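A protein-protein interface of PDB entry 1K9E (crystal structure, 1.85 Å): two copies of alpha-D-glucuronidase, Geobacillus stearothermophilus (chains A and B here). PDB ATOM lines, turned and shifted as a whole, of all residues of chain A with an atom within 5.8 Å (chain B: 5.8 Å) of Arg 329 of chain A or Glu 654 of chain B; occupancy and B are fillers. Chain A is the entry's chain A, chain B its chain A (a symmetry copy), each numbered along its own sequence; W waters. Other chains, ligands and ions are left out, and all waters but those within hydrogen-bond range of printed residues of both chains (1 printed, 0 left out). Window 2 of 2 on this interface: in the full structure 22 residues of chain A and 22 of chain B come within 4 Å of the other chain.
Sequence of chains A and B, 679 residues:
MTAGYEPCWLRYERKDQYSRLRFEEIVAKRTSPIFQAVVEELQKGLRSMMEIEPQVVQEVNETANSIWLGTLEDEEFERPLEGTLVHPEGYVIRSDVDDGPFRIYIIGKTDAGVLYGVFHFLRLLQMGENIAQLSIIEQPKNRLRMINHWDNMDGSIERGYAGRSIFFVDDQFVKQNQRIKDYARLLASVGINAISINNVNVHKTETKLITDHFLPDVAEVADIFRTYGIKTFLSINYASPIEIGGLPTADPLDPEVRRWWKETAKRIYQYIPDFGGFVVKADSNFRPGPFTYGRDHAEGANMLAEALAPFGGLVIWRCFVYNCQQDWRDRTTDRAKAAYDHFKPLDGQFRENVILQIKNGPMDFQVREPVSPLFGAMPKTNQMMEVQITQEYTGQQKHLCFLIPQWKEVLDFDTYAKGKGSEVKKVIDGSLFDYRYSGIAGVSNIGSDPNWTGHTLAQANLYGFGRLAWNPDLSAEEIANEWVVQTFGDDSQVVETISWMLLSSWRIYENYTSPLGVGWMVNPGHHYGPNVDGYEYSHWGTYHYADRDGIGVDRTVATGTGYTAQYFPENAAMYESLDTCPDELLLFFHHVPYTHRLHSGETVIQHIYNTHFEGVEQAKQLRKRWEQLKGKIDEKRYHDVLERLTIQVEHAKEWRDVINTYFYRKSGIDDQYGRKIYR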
ATOM      1  N   ASP A 327      28.499  35.822   1.691  1.00  0.00           N
ATOM      2  CA  ASP A 327      27.553  34.948   1.004  1.00  0.00           C
ATOM      3  C   ASP A 327      27.603  35.246  -0.491  1.00  0.00           C
ATOM      4  O   ASP A 327      27.293  36.358  -0.918  1.00  0.00           O
ATOM      5  CB  ASP A 327      26.134  35.189   1.524  1.00  0.00           C
ATOM      6  CG  ASP A 327      25.170  34.095   1.113  1.00  0.00           C
ATOM      7  OD1 ASP A 327      25.397  33.457   0.065  1.00  0.00           O
ATOM      8  OD2 ASP A 327      24.176  33.879   1.836  1.00  0.00           O
ATOM      9  N   TRP A 328      27.990  34.257  -1.289  1.00  0.00           N
ATOM     10  CA  TRP A 328      28.069  34.464  -2.734  1.00  0.00           C
ATOM     11  C   TRP A 328      26.725  34.853  -3.344  1.00  0.00           C
ATOM     12  O   TRP A 328      26.672  35.410  -4.440  1.00  0.00           O
ATOM     13  CB  TRP A 328      28.600  33.206  -3.434  1.00  0.00           C
ATOM     14  CG  TRP A 328      27.777  31.973  -3.215  1.00  0.00           C
ATOM     15  CD1 TRP A 328      27.980  31.006  -2.272  1.00  0.00           C
ATOM     16  CD2 TRP A 328      26.613  31.579  -3.950  1.00  0.00           C
ATOM     17  NE1 TRP A 328      27.012  30.031  -2.375  1.00  0.00           N
ATOM     18  CE2 TRP A 328      26.160  30.359  -3.397  1.00  0.00           C
ATOM     19  CE3 TRP A 328      25.905  32.139  -5.022  1.00  0.00           C
ATOM     20  CZ2 TRP A 328      25.029  29.687  -3.882  1.00  0.00           C
ATOM     21  CZ3 TRP A 328      24.775  31.469  -5.505  1.00  0.00           C
ATOM     22  CH2 TRP A 328      24.353  30.257  -4.934  1.00  0.00           C
ATOM     23  N   ARG A 329      25.643  34.553  -2.632  1.00  0.00           N
ATOM     24  CA  ARG A 329      24.292  34.865  -3.100  1.00  0.00           C
ATOM     25  C   ARG A 329      23.985  36.362  -3.049  1.00  0.00           C
ATOM     26  O   ARG A 329      23.237  36.885  -3.878  1.00  0.00           O
ATOM     27  CB  ARG A 329      23.250  34.157  -2.232  1.00  0.00           C
ATOM     28  CG  ARG A 329      23.392  32.652  -2.072  1.00  0.00           C
ATOM     29  CD  ARG A 329      22.342  32.188  -1.070  1.00  0.00           C
ATOM     30  NE  ARG A 329      22.307  30.746  -0.841  1.00  0.00           N
ATOM     31  CZ  ARG A 329      23.275  30.053  -0.250  1.00  0.00           C
ATOM     32  NH1 ARG A 329      24.372  30.665   0.171  1.00  0.00           N
ATOM     33  NH2 ARG A 329      23.127  28.750  -0.050  1.00  0.00           N
ATOM     34  N   ASP A 330      24.552  37.041  -2.059  1.00  0.00           N
ATOM     35  CA  ASP A 330      24.312  38.468  -1.861  1.00  0.00           C
ATOM     36  C   ASP A 330      25.173  39.368  -2.741  1.00  0.00           C
ATOM     37  O   ASP A 330      26.344  39.604  -2.440  1.00  0.00           O
ATOM     38  CB  ASP A 330      24.531  38.814  -0.385  1.00  0.00           C
ATOM     39  CG  ASP A 330      24.177  40.250  -0.061  1.00  0.00           C
ATOM     40  OD1 ASP A 330      23.503  40.906  -0.887  1.00  0.00           O
ATOM     41  OD2 ASP A 330      24.566  40.719   1.027  1.00  0.00           O
ATOM     42  N   ARG A 331      24.586  39.877  -3.821  1.00  0.00           N
ATOM     43  CA  ARG A 331      25.317  40.747  -4.734  1.00  0.00           C
ATOM     44  C   ARG A 331      25.360  42.205  -4.284  1.00  0.00           C
ATOM     45  O   ARG A 331      25.831  43.067  -5.025  1.00  0.00           O
ATOM     46  CB  ARG A 331      24.739  40.667  -6.156  1.00  0.00           C
ATOM     47  CG  ARG A 331      24.997  39.346  -6.879  1.00  0.00           C
ATOM     48  CD  ARG A 331      24.899  39.518  -8.396  1.00  0.00           C
ATOM     49  NE  ARG A 331      24.908  38.237  -9.102  1.00  0.00           N
ATOM     50  CZ  ARG A 331      24.979  38.104 -10.425  1.00  0.00           C
ATOM     51  NH1 ARG A 331      25.052  39.174 -11.206  1.00  0.00           N
ATOM     52  NH2 ARG A 331      24.965  36.895 -10.972  1.00  0.00           N
ATOM     53  N   TYR A 537      31.884  30.048  -5.917  1.00  0.00           N
ATOM     54  CA  TYR A 537      30.791  29.836  -4.979  1.00  0.00           C
ATOM     55  C   TYR A 537      31.333  29.719  -3.563  1.00  0.00           C
ATOM     56  O   TYR A 537      30.752  29.041  -2.714  1.00  0.00           O
ATOM     57  CB  TYR A 537      29.985  28.588  -5.340  1.00  0.00           C
ATOM     58  CG  TYR A 537      29.370  28.676  -6.715  1.00  0.00           C
ATOM     59  CD1 TYR A 537      30.092  28.303  -7.848  1.00  0.00           C
ATOM     60  CD2 TYR A 537      28.081  29.179  -6.890  1.00  0.00           C
ATOM     61  CE1 TYR A 537      29.550  28.428  -9.122  1.00  0.00           C
ATOM     62  CE2 TYR A 537      27.527  29.308  -8.161  1.00  0.00           C
ATOM     63  CZ  TYR A 537      28.265  28.933  -9.271  1.00  0.00           C
ATOM     64  OH  TYR A 537      27.723  29.076 -10.530  1.00  0.00           O
ATOM     65  N   PRO B 530      29.613  21.311  -2.071  1.00  0.00           N
ATOM     66  CA  PRO B 530      29.420  21.616  -3.489  1.00  0.00           C
ATOM     67  C   PRO B 530      30.477  22.489  -4.150  1.00  0.00           C
ATOM     68  O   PRO B 530      30.942  23.482  -3.586  1.00  0.00           O
ATOM     69  CB  PRO B 530      28.044  22.276  -3.506  1.00  0.00           C
ATOM     70  CG  PRO B 530      28.070  23.060  -2.220  1.00  0.00           C
ATOM     71  CD  PRO B 530      28.629  22.039  -1.245  1.00  0.00           C
ATOM     72  N   VAL B 649      21.075  20.124   7.524  1.00  0.00           N
ATOM     73  CA  VAL B 649      20.092  20.996   6.895  1.00  0.00           C
ATOM     74  C   VAL B 649      20.729  22.260   6.333  1.00  0.00           C
ATOM     75  O   VAL B 649      20.447  22.659   5.205  1.00  0.00           O
ATOM     76  CB  VAL B 649      18.989  21.391   7.889  1.00  0.00           C
ATOM     77  CG1 VAL B 649      18.145  22.529   7.308  1.00  0.00           C
ATOM     78  CG2 VAL B 649      18.108  20.185   8.182  1.00  0.00           C
ATOM     79  N   GLU B 650      21.589  22.896   7.117  1.00  0.00           N
ATOM     80  CA  GLU B 650      22.234  24.115   6.662  1.00  0.00           C
ATOM     81  C   GLU B 650      23.163  23.879   5.475  1.00  0.00           C
ATOM     82  O   GLU B 650      23.199  24.684   4.547  1.00  0.00           O
ATOM     83  CB  GLU B 650      22.990  24.777   7.817  1.00  0.00           C
ATOM     84  CG  GLU B 650      22.061  25.354   8.883  1.00  0.00           C
ATOM     85  CD  GLU B 650      21.046  26.326   8.295  1.00  0.00           C
ATOM     86  OE1 GLU B 650      21.462  27.370   7.745  1.00  0.00           O
ATOM     87  OE2 GLU B 650      19.833  26.039   8.370  1.00  0.00           O
ATOM     88  N   HIS B 651      23.911  22.778   5.493  1.00  0.00           N
ATOM     89  CA  HIS B 651      24.817  22.487   4.388  1.00  0.00           C
ATOM     90  C   HIS B 651      24.042  22.051   3.144  1.00  0.00           C
ATOM     91  O   HIS B 651      24.445  22.341   2.019  1.00  0.00           O
ATOM     92  CB  HIS B 651      25.817  21.398   4.791  1.00  0.00           C
ATOM     93  CG  HIS B 651      27.003  21.307   3.882  1.00  0.00           C
ATOM     94  ND1 HIS B 651      27.711  22.415   3.471  1.00  0.00           N
ATOM     95  CD2 HIS B 651      27.625  20.238   3.329  1.00  0.00           C
ATOM     96  CE1 HIS B 651      28.717  22.034   2.704  1.00  0.00           C
ATOM     97  NE2 HIS B 651      28.687  20.717   2.603  1.00  0.00           N
ATOM     98  N   ALA B 652      22.929  21.354   3.347  1.00  0.00           N
ATOM     99  CA  ALA B 652      22.109  20.911   2.222  1.00  0.00           C
ATOM    100  C   ALA B 652      21.626  22.145   1.455  1.00  0.00           C
ATOM    101  O   ALA B 652      21.508  22.121   0.228  1.00  0.00           O
ATOM    102  CB  ALA B 652      20.917  20.088   2.725  1.00  0.00           C
ATOM    103  N   LYS B 653      21.352  23.225   2.183  1.00  0.00           N
ATOM    104  CA  LYS B 653      20.901  24.465   1.556  1.00  0.00           C
ATOM    105  C   LYS B 653      21.989  25.000   0.628  1.00  0.00           C
ATOM    106  O   LYS B 653      21.698  25.556  -0.433  1.00  0.00           O
ATOM    107  CB  LYS B 653      20.563  25.517   2.622  1.00  0.00           C
ATOM    108  CG  LYS B 653      19.270  25.249   3.370  1.00  0.00           C
ATOM    109  CD  LYS B 653      19.091  26.229   4.523  1.00  0.00           C
ATOM    110  CE  LYS B 653      17.786  25.984   5.264  1.00  0.00           C
ATOM    111  NZ  LYS B 653      17.655  26.873   6.456  1.00  0.00           N
ATOM    112  N   GLU B 654      23.244  24.821   1.031  1.00  0.00           N
ATOM    113  CA  GLU B 654      24.376  25.274   0.232  1.00  0.00           C
ATOM    114  C   GLU B 654      24.480  24.393  -1.011  1.00  0.00           C
ATOM    115  O   GLU B 654      24.683  24.895  -2.111  1.00  0.00           O
ATOM    116  CB  GLU B 654      25.669  25.193   1.056  1.00  0.00           C
ATOM    117  CG  GLU B 654      26.880  25.858   0.414  1.00  0.00           C
ATOM    118  CD  GLU B 654      26.767  27.377   0.336  1.00  0.00           C
ATOM    119  OE1 GLU B 654      25.871  27.959   0.998  1.00  0.00           O
ATOM    120  OE2 GLU B 654      27.588  27.988  -0.383  1.00  0.00           O
ATOM    121  N   TRP B 655      24.343  23.079  -0.833  1.00  0.00           N
ATOM    122  CA  TRP B 655      24.385  22.149  -1.966  1.00  0.00           C
ATOM    123  C   TRP B 655      23.287  22.520  -2.970  1.00  0.00           C
ATOM    124  O   TRP B 655      23.520  22.628  -4.177  1.00  0.00           O
ATOM    125  CB  TRP B 655      24.147  20.713  -1.492  1.00  0.00           C
ATOM    126  CG  TRP B 655      25.390  19.972  -1.101  1.00  0.00           C
ATOM    127  CD1 TRP B 655      25.864  19.758   0.165  1.00  0.00           C
ATOM    128  CD2 TRP B 655      26.316  19.340  -1.991  1.00  0.00           C
ATOM    129  NE1 TRP B 655      27.031  19.022   0.115  1.00  0.00           N
ATOM    130  CE2 TRP B 655      27.331  18.756  -1.197  1.00  0.00           C
ATOM    131  CE3 TRP B 655      26.389  19.212  -3.386  1.00  0.00           C
ATOM    132  CZ2 TRP B 655      28.406  18.049  -1.753  1.00  0.00           C
ATOM    133  CZ3 TRP B 655      27.460  18.508  -3.940  1.00  0.00           C
ATOM    134  CH2 TRP B 655      28.454  17.937  -3.122  1.00  0.00           C
ATOM    135  N   ARG B 656      22.079  22.696  -2.456  1.00  0.00           N
ATOM    136  CA  ARG B 656      20.932  23.053  -3.285  1.00  0.00           C
ATOM    137  C   ARG B 656      21.182  24.301  -4.130  1.00  0.00           C
ATOM    138  O   ARG B 656      21.076  24.267  -5.362  1.00  0.00           O
ATOM    139  CB  ARG B 656      19.711  23.294  -2.393  1.00  0.00           C
ATOM    140  CG  ARG B 656      18.462  23.767  -3.128  1.00  0.00           C
ATOM    141  CD  ARG B 656      17.459  24.340  -2.135  1.00  0.00           C
ATOM    142  NE  ARG B 656      17.992  25.528  -1.466  1.00  0.00           N
ATOM    143  CZ  ARG B 656      17.534  26.007  -0.312  1.00  0.00           C
ATOM    144  NH1 ARG B 656      16.534  25.400   0.312  1.00  0.00           N
ATOM    145  NH2 ARG B 656      18.073  27.099   0.218  1.00  0.00           N
ATOM    146  N   ASP B 657      21.503  25.408  -3.464  1.00  0.00           N
ATOM    147  CA  ASP B 657      21.712  26.669  -4.162  1.00  0.00           C
ATOM    148  C   ASP B 657      22.905  26.715  -5.108  1.00  0.00           C
ATOM    149  O   ASP B 657      22.782  27.210  -6.221  1.00  0.00           O
ATOM    150  CB  ASP B 657      21.778  27.827  -3.156  1.00  0.00           C
ATOM    151  CG  ASP B 657      20.470  28.004  -2.393  1.00  0.00           C
ATOM    152  OD1 ASP B 657      19.419  27.560  -2.913  1.00  0.00           O
ATOM    153  OD2 ASP B 657      20.487  28.589  -1.286  1.00  0.00           O
ATOM    154  N   VAL B 658      24.053  26.200  -4.681  1.00  0.00           N
ATOM    155  CA  VAL B 658      25.223  26.211  -5.542  1.00  0.00           C
ATOM    156  C   VAL B 658      24.935  25.447  -6.833  1.00  0.00           C
ATOM    157  O   VAL B 658      25.184  25.946  -7.929  1.00  0.00           O
ATOM    158  CB  VAL B 658      26.446  25.580  -4.839  1.00  0.00           C
ATOM    159  CG1 VAL B 658      27.581  25.386  -5.837  1.00  0.00           C
ATOM    160  CG2 VAL B 658      26.907  26.481  -3.694  1.00  0.00           C
ATOM    161  N   ILE B 659      24.399  24.239  -6.706  1.00  0.00           N
ATOM    162  CA  ILE B 659      24.098  23.444  -7.887  1.00  0.00           C
ATOM    163  C   ILE B 659      23.005  24.083  -8.739  1.00  0.00           C
ATOM    164  O   ILE B 659      23.148  24.176  -9.957  1.00  0.00           O
ATOM    165  CB  ILE B 659      23.713  21.996  -7.499  1.00  0.00           C
ATOM    166  CG1 ILE B 659      24.970  21.271  -6.991  1.00  0.00           C
ATOM    167  CG2 ILE B 659      23.120  21.252  -8.700  1.00  0.00           C
ATOM    168  CD1 ILE B 659      24.744  19.842  -6.561  1.00  0.00           C
ATOM    169  N   TYR B 678      19.237  31.675  -6.839  1.00  0.00           N
ATOM    170  CA  TYR B 678      20.002  32.908  -6.856  1.00  0.00           C
ATOM    171  C   TYR B 678      20.725  33.018  -8.194  1.00  0.00           C
ATOM    172  O   TYR B 678      21.550  32.174  -8.543  1.00  0.00           O
ATOM    173  CB  TYR B 678      20.970  32.933  -5.673  1.00  0.00           C
ATOM    174  CG  TYR B 678      20.240  32.892  -4.345  1.00  0.00           C
ATOM    175  CD1 TYR B 678      19.888  31.678  -3.750  1.00  0.00           C
ATOM    176  CD2 TYR B 678      19.848  34.071  -3.713  1.00  0.00           C
ATOM    177  CE1 TYR B 678      19.159  31.642  -2.559  1.00  0.00           C
ATOM    178  CE2 TYR B 678      19.121  34.047  -2.529  1.00  0.00           C
ATOM    179  CZ  TYR B 678      18.779  32.833  -1.957  1.00  0.00           C
ATOM    180  OH  TYR B 678      18.052  32.818  -0.789  1.00  0.00           O
HETATM  181  O   HOH W   1      29.997  26.871  -1.022  1.00  0.00           O
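The guanidinium group of Arg 329 of chain A is in salt-bridge range of the side-chain carboxylate of Glu 654 of chain B, 3.0 Å away.
NE1 of Trp 328 of chain A lies within hydrogen-bond range of OE2 of Glu 654 of chain B.
The guanidinium group (NE) of Arg 329 of chain A is in salt-bridge range of the side-chain carboxylate (OD2) of Asp 657 of chain B (2.9 Å).
NE of Arg 656 of chain B lies within salt-bridge range of OD1 of Asp 657 of chain B, at 2.9 Å.
The side-chain carboxylate of Asp 327 of chain A is in salt-bridge range of the guanidinium group of Arg 329 of chain A, 3.0 Å away.
NZ of Lys 653 of chain B is in salt-bridge range of OE2 of Glu 650 of chain B (3.0 Å).
O of Asp 657 of chain B touches CH2 of Trp 328 of chain A, at 3.7 Å.
Val 658 of chain B touches Trp 328 of chain A.
NH2 of Arg 329 of chain A touches O of Lys 653 of chain B (3.5 Å).
CD of Arg 329 of chain A touches CE1 of Tyr 678 of chain B, at 3.6 Å.
Tyr 537 of chain A touches Val 658 of chain B (CG to CG1, 3.8 Å).
Glu 654 of chain B touches just these residues of chain A: Trp 328 and Arg 329.
Of the printed residues of chain B, Trp 328 of chain A touches Glu 654 (2.9 Å), Asp 657 (3.7 Å) and Val 658 (3.7 Å).
Printed residues of chain B within 4 Å of Tyr 537 of chain A: Val 658.
Of the printed residues of chain A, Asp 657 of chain B touches Trp 328 and Arg 329.
Printed residues of chain A within 4 Å of Tyr 678 of chain B: Arg 329.
Of the 13 printed residues of chain B, 5 touch a printed residue of chain A.
No position is printed for both chains.
Of the 8 pairs that touch across the chains among the printed residues, none has its exchanged pair printed and touching as well.
Water W1 bridges OE2 of Glu 654 of chain B (2.7 Å) and O of Tyr 537 of chain A (2.9 Å).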
